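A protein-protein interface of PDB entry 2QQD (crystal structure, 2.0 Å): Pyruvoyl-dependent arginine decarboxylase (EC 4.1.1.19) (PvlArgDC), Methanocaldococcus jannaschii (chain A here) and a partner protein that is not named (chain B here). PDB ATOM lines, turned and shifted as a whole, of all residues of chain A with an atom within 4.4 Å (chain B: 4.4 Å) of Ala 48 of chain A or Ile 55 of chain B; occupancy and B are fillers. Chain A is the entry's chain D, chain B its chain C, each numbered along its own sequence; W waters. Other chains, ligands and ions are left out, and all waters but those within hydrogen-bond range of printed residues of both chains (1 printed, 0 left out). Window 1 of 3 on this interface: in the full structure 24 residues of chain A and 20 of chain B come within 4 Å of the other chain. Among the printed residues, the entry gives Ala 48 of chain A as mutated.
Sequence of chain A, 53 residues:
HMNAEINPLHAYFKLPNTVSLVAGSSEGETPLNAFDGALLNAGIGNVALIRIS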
ATOM      1  N   GLY A  45      13.382  -9.580   7.689  1.00  0.00           N
ATOM      2  CA  GLY A  45      13.888  -8.879   8.858  1.00  0.00           C
ATOM      3  C   GLY A  45      13.972  -9.742  10.102  1.00  0.00           C
ATOM      4  O   GLY A  45      14.531  -9.313  11.110  1.00  0.00           O
ATOM      5  N   ASN A  46      13.428 -10.955  10.038  1.00  0.00           N
ATOM      6  CA  ASN A  46      13.456 -11.854  11.191  1.00  0.00           C
ATOM      7  C   ASN A  46      14.341 -13.086  10.986  1.00  0.00           C
ATOM      8  O   ASN A  46      14.072 -14.159  11.538  1.00  0.00           O
ATOM      9  CB  ASN A  46      12.028 -12.262  11.564  1.00  0.00           C
ATOM     10  CG  ASN A  46      11.256 -11.127  12.226  1.00  0.00           C
ATOM     11  OD1 ASN A  46      10.049 -10.976  12.027  1.00  0.00           O
ATOM     12  ND2 ASN A  46      11.953 -10.330  13.026  1.00  0.00           N
ATOM     13  N   VAL A  47      15.387 -12.910  10.177  1.00  0.00           N
ATOM     14  CA  VAL A  47      16.378 -13.947   9.900  1.00  0.00           C
ATOM     15  C   VAL A  47      17.756 -13.296   9.926  1.00  0.00           C
ATOM     16  O   VAL A  47      17.886 -12.075   9.810  1.00  0.00           O
ATOM     17  CB  VAL A  47      16.207 -14.606   8.489  1.00  0.00           C
ATOM     18  CG1 VAL A  47      14.985 -15.520   8.463  1.00  0.00           C
ATOM     19  CG2 VAL A  47      16.097 -13.524   7.419  1.00  0.00           C
ATOM     20  N   ALA A  48      18.783 -14.121  10.088  1.00  0.00           N
ATOM     21  CA  ALA A  48      20.153 -13.647  10.096  1.00  0.00           C
ATOM     22  C   ALA A  48      20.686 -13.790   8.677  1.00  0.00           C
ATOM     23  O   ALA A  48      20.801 -14.906   8.150  1.00  0.00           O
ATOM     24  CB  ALA A  48      20.996 -14.468  11.059  1.00  0.00           C
ATOM     25  N   LEU A  49      21.005 -12.659   8.057  1.00  0.00           N
ATOM     26  CA  LEU A  49      21.518 -12.671   6.702  1.00  0.00           C
ATOM     27  C   LEU A  49      23.023 -12.877   6.617  1.00  0.00           C
ATOM     28  O   LEU A  49      23.792 -12.158   7.252  1.00  0.00           O
ATOM     29  CB  LEU A  49      21.171 -11.361   5.999  1.00  0.00           C
ATOM     30  CG  LEU A  49      19.695 -10.947   5.916  1.00  0.00           C
ATOM     31  CD1 LEU A  49      19.608  -9.631   5.150  1.00  0.00           C
ATOM     32  CD2 LEU A  49      18.875 -12.012   5.216  1.00  0.00           C
ATOM     33  N   ILE A  50      23.446 -13.876   5.848  1.00  0.00           N
ATOM     34  CA  ILE A  50      24.871 -14.091   5.634  1.00  0.00           C
ATOM     35  C   ILE A  50      25.079 -13.480   4.250  1.00  0.00           C
ATOM     36  O   ILE A  50      24.632 -14.031   3.243  1.00  0.00           O
ATOM     37  CB  ILE A  50      25.250 -15.582   5.587  1.00  0.00           C
ATOM     38  CG1 ILE A  50      24.975 -16.233   6.945  1.00  0.00           C
ATOM     39  CG2 ILE A  50      26.743 -15.727   5.242  1.00  0.00           C
ATOM     40  CD1 ILE A  50      25.132 -17.747   6.941  1.00  0.00           C
ATOM     41  N   ILE B  52      27.046 -11.228  10.434  1.00  0.00           N
ATOM     42  CA  ILE B  52      25.666 -11.490  10.086  1.00  0.00           C
ATOM     43  C   ILE B  52      24.801 -10.322  10.453  1.00  0.00           C
ATOM     44  O   ILE B  52      25.237  -9.399  11.148  1.00  0.00           O
ATOM     45  CB  ILE B  52      25.099 -12.701  10.848  1.00  0.00           C
ATOM     46  CG1 ILE B  52      25.309 -12.503  12.351  1.00  0.00           C
ATOM     47  CG2 ILE B  52      25.747 -13.975  10.353  1.00  0.00           C
ATOM     48  CD1 ILE B  52      24.574 -13.508  13.226  1.00  0.00           C
ATOM     49  N   SER B  53      23.563 -10.383   9.979  1.00  0.00           N
ATOM     50  CA  SER B  53      22.579  -9.363  10.281  1.00  0.00           C
ATOM     51  C   SER B  53      22.286  -9.571  11.769  1.00  0.00           C
ATOM     52  O   SER B  53      22.620 -10.612  12.327  1.00  0.00           O
ATOM     53  CB  SER B  53      21.322  -9.578   9.442  1.00  0.00           C
ATOM     54  OG  SER B  53      20.804  -8.324   9.049  1.00  0.00           O
ATOM     55  N   SER B  54      21.629  -8.611  12.399  1.00  0.00           N
ATOM     56  CA  SER B  54      21.383  -8.690  13.834  1.00  0.00           C
ATOM     57  C   SER B  54      20.209  -9.511  14.390  1.00  0.00           C
ATOM     58  O   SER B  54      19.390  -8.997  15.151  1.00  0.00           O
ATOM     59  CB  SER B  54      21.332  -7.269  14.370  1.00  0.00           C
ATOM     60  OG  SER B  54      22.612  -6.653  14.279  1.00  0.00           O
ATOM     61  N   ILE B  55      20.166 -10.797  14.043  1.00  0.00           N
ATOM     62  CA  ILE B  55      19.111 -11.700  14.499  1.00  0.00           C
ATOM     63  C   ILE B  55      19.715 -12.991  15.050  1.00  0.00           C
ATOM     64  O   ILE B  55      20.690 -13.508  14.506  1.00  0.00           O
ATOM     65  CB  ILE B  55      18.162 -12.092  13.331  1.00  0.00           C
ATOM     66  CG1 ILE B  55      17.414 -10.860  12.816  1.00  0.00           C
ATOM     67  CG2 ILE B  55      17.198 -13.188  13.775  1.00  0.00           C
ATOM     68  CD1 ILE B  55      16.540 -10.182  13.848  1.00  0.00           C
ATOM     69  N   MET B  56      19.143 -13.506  16.136  1.00  0.00           N
ATOM     70  CA  MET B  56      19.620 -14.754  16.711  1.00  0.00           C
ATOM     71  C   MET B  56      18.452 -15.735  16.821  1.00  0.00           C
ATOM     72  O   MET B  56      17.301 -15.331  16.988  1.00  0.00           O
ATOM     73  CB  MET B  56      20.263 -14.527  18.086  1.00  0.00           C
ATOM     74  CG  MET B  56      19.323 -14.036  19.169  1.00  0.00           C
ATOM     75  SD  MET B  56      20.182 -13.916  20.755  1.00  0.00           S
ATOM     76  CE  MET B  56      19.254 -15.115  21.762  1.00  0.00           C
ATOM     77  N   CYS B 105      12.450 -14.851  17.264  1.00  0.00           N
ATOM     78  CA  CYS B 105      13.899 -14.724  17.282  1.00  0.00           C
ATOM     79  C   CYS B 105      14.332 -13.601  18.221  1.00  0.00           C
ATOM     80  O   CYS B 105      13.521 -12.771  18.615  1.00  0.00           O
ATOM     81  CB  CYS B 105      14.416 -14.440  15.870  1.00  0.00           C
ATOM     82  SG  CYS B 105      13.720 -12.941  15.122  1.00  0.00           S
ATOM     83  N   GLY B 106      15.611 -13.597  18.587  1.00  0.00           N
ATOM     84  CA  GLY B 106      16.124 -12.553  19.452  1.00  0.00           C
ATOM     85  C   GLY B 106      16.734 -11.486  18.564  1.00  0.00           C
ATOM     86  O   GLY B 106      17.169 -11.795  17.449  1.00  0.00           O
ATOM     87  N   LEU B 107      16.763 -10.242  19.031  1.00  0.00           N
ATOM     88  CA  LEU B 107      17.346  -9.156  18.244  1.00  0.00           C
ATOM     89  C   LEU B 107      18.715  -8.749  18.760  1.00  0.00           C
ATOM     90  O   LEU B 107      18.940  -8.674  19.961  1.00  0.00           O
ATOM     91  CB  LEU B 107      16.464  -7.907  18.269  1.00  0.00           C
ATOM     92  CG  LEU B 107      15.074  -7.937  17.640  1.00  0.00           C
ATOM     93  CD1 LEU B 107      14.525  -6.513  17.620  1.00  0.00           C
ATOM     94  CD2 LEU B 107      15.149  -8.498  16.228  1.00  0.00           C
ATOM     95  N   ARG B 135       8.477  -4.120  15.674  1.00  0.00           N
ATOM     96  CA  ARG B 135       7.890  -5.431  15.391  1.00  0.00           C
ATOM     97  C   ARG B 135       6.579  -5.625  16.157  1.00  0.00           C
ATOM     98  O   ARG B 135       5.729  -6.425  15.761  1.00  0.00           O
ATOM     99  CB  ARG B 135       8.881  -6.553  15.754  1.00  0.00           C
ATOM    100  CG  ARG B 135      10.053  -6.696  14.780  1.00  0.00           C
ATOM    101  CD  ARG B 135      11.061  -7.742  15.257  1.00  0.00           C
ATOM    102  NE  ARG B 135      12.140  -7.979  14.298  1.00  0.00           N
ATOM    103  CZ  ARG B 135      13.091  -7.100  13.995  1.00  0.00           C
ATOM    104  NH1 ARG B 135      13.107  -5.907  14.575  1.00  0.00           N
ATOM    105  NH2 ARG B 135      14.034  -7.418  13.116  1.00  0.00           N
ATOM    106  N   LEU B 163      27.564 -16.139  17.886  1.00  0.00           N
ATOM    107  CA  LEU B 163      26.642 -17.265  17.977  1.00  0.00           C
ATOM    108  C   LEU B 163      27.386 -18.595  17.849  1.00  0.00           C
ATOM    109  O   LEU B 163      28.163 -18.795  16.925  1.00  0.00           O
ATOM    110  CB  LEU B 163      25.588 -17.174  16.868  1.00  0.00           C
ATOM    111  CG  LEU B 163      24.756 -15.895  16.736  1.00  0.00           C
ATOM    112  CD1 LEU B 163      23.714 -16.094  15.626  1.00  0.00           C
ATOM    113  CD2 LEU B 163      24.059 -15.570  18.068  1.00  0.00           C
HETATM  114  O   HOH W   1      18.188  -9.483   9.719  1.00  0.00           O
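The side-chain amide nitrogen of Asn 46 of chain A sits close to the guanidinium group of Arg 135 of chain B. The guanidinium group of Arg 135 of chain B lies within hydrogen-bond range of the backbone carbonyl oxygen of Gly 45 of chain A, 2.8 Å away. The side-chain amide nitrogen (ND2) of Asn 46 of chain A lies within hydrogen-bond range of the side-chain sulfur (SG) of Cys 105 of chain B (3.8 Å). The backbone carbonyl oxygen (O) of Leu 49 of chain A sits at hydrogen-bond distance from the backbone NH (N) of Ser 53 of chain B (3.3 Å).
Ile 55 of chain B touches Gly 45 of chain A. CG2 of Ile 55 of chain B touches O of Asn 46 of chain A, 3.96 Å away. Ile 55 of chain B touches Val 47 of chain A (CG1 to O, 3.3 Å). Ala 48 of chain A touches Ile 55 of chain B. Leu 49 of chain A touches Ile 52 of chain B (O to CA, 3.5 Å).
Ala 48 of chain A touches one residue of chain B. Ile 55 of chain B touches just these residues of chain A: Gly 45, Asn 46, Val 47 and Ala 48. Of the printed residues of chain A, Ser 53 of chain B touches Leu 49. Of the printed residues of chain A, Cys 105 of chain B touches Asn 46 (3.8 Å). The nearest printed residue of chain A that does not touch Cys 105 of chain B is Val 47 of chain A (5.2 Å).
Of the 6 printed residues of chain A, 5 touch a printed residue of chain B. Among the printed residues, no Asp or Glu carboxylate lies within 4 Å of a Lys or Arg side-chain nitrogen of the other chain.
Water W1 lies within hydrogen-bond range of the backbone carbonyl oxygen of Val 47 of chain A and the side-chain hydroxyl of Ser 53 of chain B.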
